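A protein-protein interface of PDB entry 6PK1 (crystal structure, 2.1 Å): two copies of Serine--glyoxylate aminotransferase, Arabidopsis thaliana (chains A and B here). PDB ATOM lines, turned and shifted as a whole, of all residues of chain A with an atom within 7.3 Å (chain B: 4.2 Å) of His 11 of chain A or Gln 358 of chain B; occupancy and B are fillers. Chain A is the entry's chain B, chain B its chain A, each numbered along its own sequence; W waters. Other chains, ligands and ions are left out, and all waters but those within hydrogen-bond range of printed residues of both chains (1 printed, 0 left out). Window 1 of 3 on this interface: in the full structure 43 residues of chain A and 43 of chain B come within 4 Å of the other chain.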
ATOM      1  N   PRO A   7      31.276  20.007  30.291  1.00  0.00           N
ATOM      2  CA  PRO A   7      30.589  21.286  30.510  1.00  0.00           C
ATOM      3  C   PRO A   7      29.760  21.721  29.314  1.00  0.00           C
ATOM      4  O   PRO A   7      30.098  21.448  28.173  1.00  0.00           O
ATOM      5  CB  PRO A   7      31.739  22.290  30.770  1.00  0.00           C
ATOM      6  CG  PRO A   7      32.891  21.429  31.168  1.00  0.00           C
ATOM      7  CD  PRO A   7      32.742  20.149  30.411  1.00  0.00           C
ATOM      8  N   GLY A   8      28.653  22.439  29.598  1.00  0.00           N
ATOM      9  CA  GLY A   8      27.866  23.066  28.567  1.00  0.00           C
ATOM     10  C   GLY A   8      27.048  22.015  27.825  1.00  0.00           C
ATOM     11  O   GLY A   8      26.977  20.851  28.205  1.00  0.00           O
ATOM     12  N   ARG A   9      26.404  22.460  26.748  1.00  0.00           N
ATOM     13  CA  ARG A   9      25.583  21.541  25.973  1.00  0.00           C
ATOM     14  C   ARG A   9      26.467  20.790  24.979  1.00  0.00           C
ATOM     15  O   ARG A   9      27.392  21.372  24.356  1.00  0.00           O
ATOM     16  CB  ARG A   9      24.454  22.252  25.235  1.00  0.00           C
ATOM     17  CG  ARG A   9      23.279  22.726  26.136  1.00  0.00           C
ATOM     18  CD  ARG A   9      22.422  21.596  26.764  1.00  0.00           C
ATOM     19  NE  ARG A   9      22.914  21.158  28.084  1.00  0.00           N
ATOM     20  CZ  ARG A   9      23.277  19.907  28.399  1.00  0.00           C
ATOM     21  NH1 ARG A   9      23.195  18.928  27.499  1.00  0.00           N
ATOM     22  NH2 ARG A   9      23.726  19.634  29.621  1.00  0.00           N
ATOM     23  N   HIS A  10      26.158  19.496  24.820  1.00  0.00           N
ATOM     24  CA  HIS A  10      26.862  18.657  23.866  1.00  0.00           C
ATOM     25  C   HIS A  10      26.438  19.031  22.454  1.00  0.00           C
ATOM     26  O   HIS A  10      25.249  19.259  22.177  1.00  0.00           O
ATOM     27  CB  HIS A  10      26.586  17.167  24.129  1.00  0.00           C
ATOM     28  CG  HIS A  10      27.178  16.259  23.112  1.00  0.00           C
ATOM     29  ND1 HIS A  10      28.532  16.030  23.037  1.00  0.00           N
ATOM     30  CD2 HIS A  10      26.621  15.560  22.096  1.00  0.00           C
ATOM     31  CE1 HIS A  10      28.791  15.210  22.032  1.00  0.00           C
ATOM     32  NE2 HIS A  10      27.647  14.901  21.447  1.00  0.00           N
ATOM     33  N   HIS A  11      27.427  19.153  21.563  1.00  0.00           N
ATOM     34  CA  HIS A  11      27.160  19.519  20.180  1.00  0.00           C
ATOM     35  C   HIS A  11      27.086  18.246  19.347  1.00  0.00           C
ATOM     36  O   HIS A  11      28.113  17.628  19.025  1.00  0.00           O
ATOM     37  CB  HIS A  11      28.250  20.477  19.725  1.00  0.00           C
ATOM     38  CG  HIS A  11      28.358  21.687  20.595  1.00  0.00           C
ATOM     39  ND1 HIS A  11      27.623  22.822  20.364  1.00  0.00           N
ATOM     40  CD2 HIS A  11      29.075  21.919  21.719  1.00  0.00           C
ATOM     41  CE1 HIS A  11      27.963  23.739  21.247  1.00  0.00           C
ATOM     42  NE2 HIS A  11      28.821  23.210  22.098  1.00  0.00           N
ATOM     43  N   LEU A  12      25.862  17.895  18.973  1.00  0.00           N
ATOM     44  CA  LEU A  12      25.553  16.657  18.276  1.00  0.00           C
ATOM     45  C   LEU A  12      25.514  16.905  16.776  1.00  0.00           C
ATOM     46  O   LEU A  12      24.492  17.340  16.241  1.00  0.00           O
ATOM     47  CB  LEU A  12      24.207  16.131  18.771  1.00  0.00           C
ATOM     48  CG  LEU A  12      23.805  14.743  18.266  1.00  0.00           C
ATOM     49  CD1 LEU A  12      24.686  13.643  18.826  1.00  0.00           C
ATOM     50  CD2 LEU A  12      22.320  14.501  18.586  1.00  0.00           C
ATOM     51  N   PHE A  13      26.612  16.605  16.081  1.00  0.00           N
ATOM     52  CA  PHE A  13      26.724  16.841  14.638  1.00  0.00           C
ATOM     53  C   PHE A  13      27.078  15.574  13.874  1.00  0.00           C
ATOM     54  O   PHE A  13      27.734  15.611  12.836  1.00  0.00           O
ATOM     55  CB  PHE A  13      27.683  17.995  14.353  1.00  0.00           C
ATOM     56  CG  PHE A  13      27.016  19.333  14.615  1.00  0.00           C
ATOM     57  CD1 PHE A  13      26.997  19.865  15.902  1.00  0.00           C
ATOM     58  CD2 PHE A  13      26.324  19.986  13.626  1.00  0.00           C
ATOM     59  CE1 PHE A  13      26.336  21.027  16.167  1.00  0.00           C
ATOM     60  CE2 PHE A  13      25.668  21.163  13.885  1.00  0.00           C
ATOM     61  CZ  PHE A  13      25.663  21.678  15.149  1.00  0.00           C
ATOM     62  N   VAL A  14      26.517  14.452  14.315  1.00  0.00           N
ATOM     63  CA  VAL A  14      26.488  13.207  13.548  1.00  0.00           C
ATOM     64  C   VAL A  14      25.208  13.211  12.721  1.00  0.00           C
ATOM     65  O   VAL A  14      24.171  13.786  13.132  1.00  0.00           O
ATOM     66  CB  VAL A  14      26.601  11.963  14.442  1.00  0.00           C
ATOM     67  CG1 VAL A  14      28.022  11.956  15.053  1.00  0.00           C
ATOM     68  CG2 VAL A  14      25.506  11.960  15.542  1.00  0.00           C
ATOM     69  N   ASN A  19      19.407  16.091  16.809  1.00  0.00           N
ATOM     70  CA  ASN A  19      18.874  16.819  17.939  1.00  0.00           C
ATOM     71  C   ASN A  19      17.359  16.737  17.962  1.00  0.00           C
ATOM     72  O   ASN A  19      16.707  16.830  16.924  1.00  0.00           O
ATOM     73  CB  ASN A  19      19.310  18.261  17.871  1.00  0.00           C
ATOM     74  CG  ASN A  19      20.804  18.426  18.117  1.00  0.00           C
ATOM     75  OD1 ASN A  19      21.286  18.345  19.269  1.00  0.00           O
ATOM     76  ND2 ASN A  19      21.548  18.590  17.042  1.00  0.00           N
ATOM     77  N   ALA A 326      37.423  16.034  18.940  1.00  0.00           N
ATOM     78  CA  ALA A 326      36.152  16.735  19.093  1.00  0.00           C
ATOM     79  C   ALA A 326      35.403  16.284  20.333  1.00  0.00           C
ATOM     80  O   ALA A 326      34.811  17.110  21.040  1.00  0.00           O
ATOM     81  CB  ALA A 326      35.267  16.503  17.874  1.00  0.00           C
ATOM     82  N   TRP A 327      35.393  14.977  20.585  1.00  0.00           N
ATOM     83  CA  TRP A 327      34.733  14.392  21.749  1.00  0.00           C
ATOM     84  C   TRP A 327      35.468  14.703  23.047  1.00  0.00           C
ATOM     85  O   TRP A 327      34.844  15.095  24.029  1.00  0.00           O
ATOM     86  CB  TRP A 327      34.645  12.870  21.557  1.00  0.00           C
ATOM     87  CG  TRP A 327      34.188  12.096  22.717  1.00  0.00           C
ATOM     88  CD1 TRP A 327      34.942  11.309  23.529  1.00  0.00           C
ATOM     89  CD2 TRP A 327      32.862  12.028  23.216  1.00  0.00           C
ATOM     90  NE1 TRP A 327      34.185  10.776  24.511  1.00  0.00           N
ATOM     91  CE2 TRP A 327      32.891  11.191  24.342  1.00  0.00           C
ATOM     92  CE3 TRP A 327      31.651  12.592  22.823  1.00  0.00           C
ATOM     93  CZ2 TRP A 327      31.740  10.880  25.076  1.00  0.00           C
ATOM     94  CZ3 TRP A 327      30.512  12.295  23.554  1.00  0.00           C
ATOM     95  CH2 TRP A 327      30.559  11.446  24.658  1.00  0.00           C
ATOM     96  N   TYR A 330      36.196  19.215  23.014  1.00  0.00           N
ATOM     97  CA  TYR A 330      35.275  20.254  22.563  1.00  0.00           C
ATOM     98  C   TYR A 330      33.822  19.876  22.798  1.00  0.00           C
ATOM     99  O   TYR A 330      32.921  20.673  22.444  1.00  0.00           O
ATOM    100  CB  TYR A 330      35.469  20.584  21.080  1.00  0.00           C
ATOM    101  CG  TYR A 330      36.898  21.113  20.793  1.00  0.00           C
ATOM    102  CD1 TYR A 330      37.239  22.438  21.052  1.00  0.00           C
ATOM    103  CD2 TYR A 330      37.845  20.298  20.276  1.00  0.00           C
ATOM    104  CE1 TYR A 330      38.493  22.921  20.830  1.00  0.00           C
ATOM    105  CE2 TYR A 330      39.171  20.775  20.029  1.00  0.00           C
ATOM    106  CZ  TYR A 330      39.467  22.074  20.314  1.00  0.00           C
ATOM    107  OH  TYR A 330      40.703  22.547  20.101  1.00  0.00           O
ATOM    108  N   ASN A 331      33.574  18.682  23.367  1.00  0.00           N
ATOM    109  CA  ASN A 331      32.220  18.223  23.655  1.00  0.00           C
ATOM    110  C   ASN A 331      31.374  18.273  22.383  1.00  0.00           C
ATOM    111  O   ASN A 331      30.291  18.830  22.344  1.00  0.00           O
ATOM    112  CB  ASN A 331      31.582  19.070  24.756  1.00  0.00           C
ATOM    113  CG  ASN A 331      30.468  18.330  25.464  1.00  0.00           C
ATOM    114  OD1 ASN A 331      30.107  17.200  25.084  1.00  0.00           O
ATOM    115  ND2 ASN A 331      29.943  18.936  26.493  1.00  0.00           N
ATOM    116  N   LEU A 332      31.919  17.713  21.328  1.00  0.00           N
ATOM    117  CA  LEU A 332      31.411  17.780  19.970  1.00  0.00           C
ATOM    118  C   LEU A 332      31.460  16.353  19.418  1.00  0.00           C
ATOM    119  O   LEU A 332      32.489  15.661  19.525  1.00  0.00           O
ATOM    120  CB  LEU A 332      32.257  18.718  19.080  1.00  0.00           C
ATOM    121  CG  LEU A 332      31.997  18.707  17.588  1.00  0.00           C
ATOM    122  CD1 LEU A 332      30.625  19.164  17.195  1.00  0.00           C
ATOM    123  CD2 LEU A 332      33.051  19.588  16.841  1.00  0.00           C
ATOM    124  N   SER A 333      30.352  15.925  18.827  1.00  0.00           N
ATOM    125  CA  SER A 333      30.213  14.626  18.174  1.00  0.00           C
ATOM    126  C   SER A 333      30.204  14.854  16.683  1.00  0.00           C
ATOM    127  O   SER A 333      29.348  15.587  16.191  1.00  0.00           O
ATOM    128  CB  SER A 333      28.908  13.958  18.629  1.00  0.00           C
ATOM    129  OG  SER A 333      29.218  13.309  19.788  1.00  0.00           O
ATOM    130  N   LEU A 334      31.171  14.273  15.978  1.00  0.00           N
ATOM    131  CA  LEU A 334      31.225  14.275  14.520  1.00  0.00           C
ATOM    132  C   LEU A 334      31.189  12.830  13.986  1.00  0.00           C
ATOM    133  O   LEU A 334      31.513  11.880  14.691  1.00  0.00           O
ATOM    134  CB  LEU A 334      32.512  14.961  14.007  1.00  0.00           C
ATOM    135  CG  LEU A 334      32.739  16.429  14.332  1.00  0.00           C
ATOM    136  CD1 LEU A 334      34.137  16.816  13.949  1.00  0.00           C
ATOM    137  CD2 LEU A 334      31.685  17.285  13.636  1.00  0.00           C
ATOM    138  N   LEU A 357      23.160  29.288  13.993  1.00  0.00           N
ATOM    139  CA  LEU A 357      24.188  29.569  14.985  1.00  0.00           C
ATOM    140  C   LEU A 357      24.747  28.290  15.623  1.00  0.00           C
ATOM    141  O   LEU A 357      25.918  28.271  16.044  1.00  0.00           O
ATOM    142  CB  LEU A 357      23.687  30.497  16.058  1.00  0.00           C
ATOM    143  CG  LEU A 357      23.306  31.910  15.617  1.00  0.00           C
ATOM    144  CD1 LEU A 357      23.338  32.884  16.833  1.00  0.00           C
ATOM    145  CD2 LEU A 357      24.045  32.429  14.543  1.00  0.00           C
ATOM    146  N   GLN A 358      23.926  27.231  15.737  1.00  0.00           N
ATOM    147  CA  GLN A 358      24.438  25.927  16.155  1.00  0.00           C
ATOM    148  C   GLN A 358      25.479  25.414  15.178  1.00  0.00           C
ATOM    149  O   GLN A 358      26.566  24.966  15.570  1.00  0.00           O
ATOM    150  CB  GLN A 358      23.322  24.890  16.263  1.00  0.00           C
ATOM    151  CG  GLN A 358      22.426  25.084  17.485  1.00  0.00           C
ATOM    152  CD  GLN A 358      21.199  24.143  17.406  1.00  0.00           C
ATOM    153  OE1 GLN A 358      20.203  24.397  16.726  1.00  0.00           O
ATOM    154  NE2 GLN A 358      21.306  23.054  18.085  1.00  0.00           N
ATOM    155  N   GLY A 361      28.786  27.410  15.428  1.00  0.00           N
ATOM    156  CA  GLY A 361      29.577  26.951  16.553  1.00  0.00           C
ATOM    157  C   GLY A 361      30.340  25.684  16.229  1.00  0.00           C
ATOM    158  O   GLY A 361      31.502  25.518  16.626  1.00  0.00           O
ATOM    159  N   CYS A 362      29.692  24.758  15.520  1.00  0.00           N
ATOM    160  CA  CYS A 362      30.397  23.535  15.129  1.00  0.00           C
ATOM    161  C   CYS A 362      31.576  23.851  14.205  1.00  0.00           C
ATOM    162  O   CYS A 362      32.701  23.358  14.387  1.00  0.00           O
ATOM    163  CB  CYS A 362      29.432  22.562  14.486  1.00  0.00           C
ATOM    164  SG  CYS A 362      30.195  21.143  13.698  1.00  0.00           S
ATOM    165  N   ARG B   9      17.815  24.999  18.604  1.00  0.00           N
ATOM    166  CA  ARG B   9      17.916  25.370  20.009  1.00  0.00           C
ATOM    167  C   ARG B   9      18.145  26.880  20.097  1.00  0.00           C
ATOM    168  O   ARG B   9      18.962  27.449  19.333  1.00  0.00           O
ATOM    169  CB  ARG B   9      19.043  24.589  20.689  1.00  0.00           C
ATOM    170  CG  ARG B   9      18.898  24.380  22.199  1.00  0.00           C
ATOM    171  CD  ARG B   9      20.200  23.809  22.804  1.00  0.00           C
ATOM    172  NE  ARG B   9      21.378  24.579  22.377  1.00  0.00           N
ATOM    173  CZ  ARG B   9      22.619  24.105  22.297  1.00  0.00           C
ATOM    174  NH1 ARG B   9      22.876  22.850  22.630  1.00  0.00           N
ATOM    175  NH2 ARG B   9      23.595  24.891  21.871  1.00  0.00           N
ATOM    176  N   PHE B  13      21.959  33.971  25.731  1.00  0.00           N
ATOM    177  CA  PHE B  13      23.194  34.667  26.088  1.00  0.00           C
ATOM    178  C   PHE B  13      22.909  35.956  26.823  1.00  0.00           C
ATOM    179  O   PHE B  13      23.651  36.932  26.701  1.00  0.00           O
ATOM    180  CB  PHE B  13      24.084  34.850  24.850  1.00  0.00           C
ATOM    181  CG  PHE B  13      24.805  33.559  24.505  1.00  0.00           C
ATOM    182  CD1 PHE B  13      24.196  32.591  23.703  1.00  0.00           C
ATOM    183  CD2 PHE B  13      26.023  33.256  25.074  1.00  0.00           C
ATOM    184  CE1 PHE B  13      24.827  31.388  23.421  1.00  0.00           C
ATOM    185  CE2 PHE B  13      26.637  32.039  24.790  1.00  0.00           C
ATOM    186  CZ  PHE B  13      26.033  31.123  23.977  1.00  0.00           C
ATOM    187  N   VAL B 354      27.921  26.665  30.213  1.00  0.00           N
ATOM    188  CA  VAL B 354      28.048  26.997  28.800  1.00  0.00           C
ATOM    189  C   VAL B 354      29.484  26.686  28.381  1.00  0.00           C
ATOM    190  O   VAL B 354      30.405  26.852  29.163  1.00  0.00           O
ATOM    191  CB  VAL B 354      27.636  28.465  28.564  1.00  0.00           C
ATOM    192  CG1 VAL B 354      28.531  29.436  29.322  1.00  0.00           C
ATOM    193  CG2 VAL B 354      27.742  28.812  27.107  1.00  0.00           C
ATOM    194  N   ASN B 355      29.684  26.133  27.191  1.00  0.00           N
ATOM    195  CA  ASN B 355      31.021  25.815  26.735  1.00  0.00           C
ATOM    196  C   ASN B 355      31.435  26.728  25.582  1.00  0.00           C
ATOM    197  O   ASN B 355      30.686  27.588  25.089  1.00  0.00           O
ATOM    198  CB  ASN B 355      31.112  24.337  26.376  1.00  0.00           C
ATOM    199  CG  ASN B 355      30.145  23.891  25.282  1.00  0.00           C
ATOM    200  OD1 ASN B 355      29.907  24.570  24.255  1.00  0.00           O
ATOM    201  ND2 ASN B 355      29.549  22.740  25.525  1.00  0.00           N
ATOM    202  N   GLU B 356      32.635  26.478  25.100  1.00  0.00           N
ATOM    203  CA  GLU B 356      33.295  27.367  24.136  1.00  0.00           C
ATOM    204  C   GLU B 356      32.631  27.385  22.762  1.00  0.00           C
ATOM    205  O   GLU B 356      32.511  28.455  22.159  1.00  0.00           O
ATOM    206  CB  GLU B 356      34.754  26.939  23.989  1.00  0.00           C
ATOM    207  CG  GLU B 356      35.650  27.295  25.144  1.00  0.00           C
ATOM    208  CD  GLU B 356      35.613  26.281  26.298  1.00  0.00           C
ATOM    209  OE1 GLU B 356      34.930  25.229  26.181  1.00  0.00           O
ATOM    210  OE2 GLU B 356      36.296  26.552  27.308  1.00  0.00           O
ATOM    211  N   LEU B 357      32.193  26.219  22.244  1.00  0.00           N
ATOM    212  CA  LEU B 357      31.494  26.224  20.967  1.00  0.00           C
ATOM    213  C   LEU B 357      30.153  26.972  21.045  1.00  0.00           C
ATOM    214  O   LEU B 357      29.744  27.581  20.052  1.00  0.00           O
ATOM    215  CB  LEU B 357      31.278  24.813  20.474  1.00  0.00           C
ATOM    216  CG  LEU B 357      32.490  23.914  20.180  1.00  0.00           C
ATOM    217  CD1 LEU B 357      32.187  22.862  19.168  1.00  0.00           C
ATOM    218  CD2 LEU B 357      33.711  24.604  19.882  1.00  0.00           C
ATOM    219  N   GLN B 358      29.431  26.891  22.177  1.00  0.00           N
ATOM    220  CA  GLN B 358      28.224  27.700  22.352  1.00  0.00           C
ATOM    221  C   GLN B 358      28.559  29.177  22.215  1.00  0.00           C
ATOM    222  O   GLN B 358      27.891  29.908  21.490  1.00  0.00           O
ATOM    223  CB  GLN B 358      27.561  27.441  23.714  1.00  0.00           C
ATOM    224  CG  GLN B 358      26.857  26.069  23.803  1.00  0.00           C
ATOM    225  CD  GLN B 358      26.331  25.775  25.211  1.00  0.00           C
ATOM    226  OE1 GLN B 358      27.035  25.263  26.064  1.00  0.00           O
ATOM    227  NE2 GLN B 358      25.090  26.114  25.442  1.00  0.00           N
ATOM    228  N   LEU B 359      29.582  29.638  22.937  1.00  0.00           N
ATOM    229  CA  LEU B 359      29.994  31.030  22.852  1.00  0.00           C
ATOM    230  C   LEU B 359      30.387  31.401  21.426  1.00  0.00           C
ATOM    231  O   LEU B 359      29.977  32.438  20.914  1.00  0.00           O
ATOM    232  CB  LEU B 359      31.142  31.279  23.829  1.00  0.00           C
ATOM    233  CG  LEU B 359      31.651  32.720  23.757  1.00  0.00           C
ATOM    234  CD1 LEU B 359      30.595  33.645  24.420  1.00  0.00           C
ATOM    235  CD2 LEU B 359      32.975  32.799  24.451  1.00  0.00           C
ATOM    236  N   LEU B 360      31.178  30.570  20.758  1.00  0.00           N
ATOM    237  CA  LEU B 360      31.604  30.909  19.397  1.00  0.00           C
ATOM    238  C   LEU B 360      30.420  31.003  18.447  1.00  0.00           C
ATOM    239  O   LEU B 360      30.408  31.849  17.566  1.00  0.00           O
ATOM    240  CB  LEU B 360      32.624  29.887  18.859  1.00  0.00           C
ATOM    241  CG  LEU B 360      33.983  29.956  19.531  1.00  0.00           C
ATOM    242  CD1 LEU B 360      34.857  28.817  19.138  1.00  0.00           C
ATOM    243  CD2 LEU B 360      34.682  31.275  19.179  1.00  0.00           C
ATOM    244  N   GLY B 361      29.398  30.175  18.615  1.00  0.00           N
ATOM    245  CA  GLY B 361      28.205  30.349  17.806  1.00  0.00           C
ATOM    246  C   GLY B 361      27.551  31.697  18.063  1.00  0.00           C
ATOM    247  O   GLY B 361      27.139  32.384  17.127  1.00  0.00           O
ATOM    248  N   CYS B 362      27.458  32.107  19.336  1.00  0.00           N
ATOM    249  CA  CYS B 362      26.936  33.441  19.631  1.00  0.00           C
ATOM    250  C   CYS B 362      27.777  34.536  18.950  1.00  0.00           C
ATOM    251  O   CYS B 362      27.241  35.449  18.293  1.00  0.00           O
ATOM    252  CB  CYS B 362      26.898  33.645  21.125  1.00  0.00           C
ATOM    253  SG  CYS B 362      26.514  35.337  21.575  1.00  0.00           S
HETATM  254  O   HOH W   1      33.028  23.377  23.626  1.00  0.00           O
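Printed residues of chain A that touch a printed residue of chain B: Pro 7, Gly 8, Arg 9, His 11, Tyr 330, Asn 331, Leu 357, Gln 358 and Gly 361. Hydrophobic or aromatic side chains of chain A within 4 Å of the printed part of chain B: His 11 and Leu 357. Along chain A the printed residues that touch a printed residue of chain B span positions 7 to 361. Of the 11 printed residues of chain B, 6 touch a printed residue of chain A. Hydrophobic or aromatic side chains of chain B that line the printed part of chain A: Leu 357. Along chain B the printed residues that touch a printed residue of chain A span positions 9 to 361. Among the printed residues, 16 pairs touch across the chains. Among the printed residues, no Asp or Glu carboxylate lies within 4 Å of a Lys or Arg side-chain nitrogen of the other chain.
Of chain A, only Gly 8 (3.4 Å), Arg 9 (3.0 Å) and His 11 (3.6 Å) come within 4 Å of Gln 358 of chain B. Of the printed residues of chain B, Pro 7 of chain A touches Asn 355 (3.0 Å). Of the printed residues of chain B, Arg 9 of chain A touches Arg 9 (3.1 Å), Asn 355 (2.8 Å) and Gln 358 (3.0 Å). Of the printed residues of chain A, Asn 355 of chain B touches Pro 7, Gly 8, Arg 9, His 11 and Asn 331. Of the printed residues of chain B, Gln 358 of chain A touches Arg 9 (3.1 Å). Cys 362 of chain B touches none of the printed residues of chain A. Leu 332 of chain A touches none of the printed residues of chain B. The nearest residue of chain A that does not touch Gln 358 of chain B is Pro 7 of chain A (5.3 Å).
Gly 8 of chain A touches Val 354 of chain B. Asn 355 of chain B touches Gly 8 of chain A. Arg 9 of chain A touches Arg 9 of chain B (CB to NH1, 3.1 Å). CB of Leu 357 of chain B touches NE2 of His 11 of chain A, 3.4 Å away. CE1 of His 11 of chain A touches N of Gln 358 of chain B, 3.6 Å away. Tyr 330 of chain A touches Leu 357 of chain B (O to CG, 3.98 Å). Asn 355 of chain B touches Asn 331 of chain A. CA of Gly 361 of chain B touches O of Leu 357 of chain A, 3.6 Å away. CA of Gly 361 of chain A touches O of Leu 357 of chain B, at 3.6 Å. Gly 361 of chain A touches Gly 361 of chain B (N to CA, 3.8 Å).
Water W1 lies within hydrogen-bond range of O of Tyr 330 of chain A (3.0 Å), N of Leu 357 of chain B (3.3 Å), OD1 of Asn 355 of chain B (3.4 Å) and N of Glu 356 of chain B (3.5 Å).
N of Arg 9 of chain B lies within hydrogen-bond range of OE1 of Gln 358 of chain A (3.1 Å). The backbone carbonyl oxygen (O) of Pro 7 of chain A sits at hydrogen-bond distance from the side-chain amide nitrogen (ND2) of Asn 355 of chain B, at 3.0 Å. The side-chain amide nitrogen of Asn 355 of chain B lies within hydrogen-bond range of the backbone carbonyl oxygen of Arg 9 of chain A, at 2.8 Å. OD1 of Asn 355 of chain B is in hydrogen-bond range of NE2 of His 11 of chain A (2.8 Å). OE1 of Gln 358 of chain B sits at hydrogen-bond distance from N of Arg 9 of chain A, at 3.0 Å.
Arg 9 of chain A touches its own counterpart, Arg 9 of chain B. Arg 9 of chain A touches Gln 358 of chain B, and with the chains exchanged Gln 358 of chain A touches Arg 9 of chain B. Leu 357 of chain A touches Gly 361 of chain B, and with the chains exchanged Gly 361 of chain A touches Leu 357 of chain B. Gly 361 of chain B touches its own counterpart, Gly 361 of chain A.
N of Leu 357 of chain B lies close to OD1 of Asn 355 of chain B (3.5 Å). The backbone carbonyl oxygen (O) of Pro 7 of chain A lies within hydrogen-bond range of the side-chain amide nitrogen (ND2) of Asn 331 of chain A (3.0 Å). ND1 of His 10 of chain A sits at hydrogen-bond distance from OD1 of Asn 331 of chain A (2.8 Å). The backbone NH (N) of His 11 of chain A lies within hydrogen-bond range of the backbone carbonyl oxygen (O) of Asn 331 of chain A, at 3.0 Å. The backbone carbonyl oxygen (O) of His 11 of chain A sits at hydrogen-bond distance from the backbone NH (N) of Ser 333 of chain A (2.8 Å). N of Asn 331 of chain A is in hydrogen-bond range of O of Ala 326 of chain A, 3.1 Å away.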
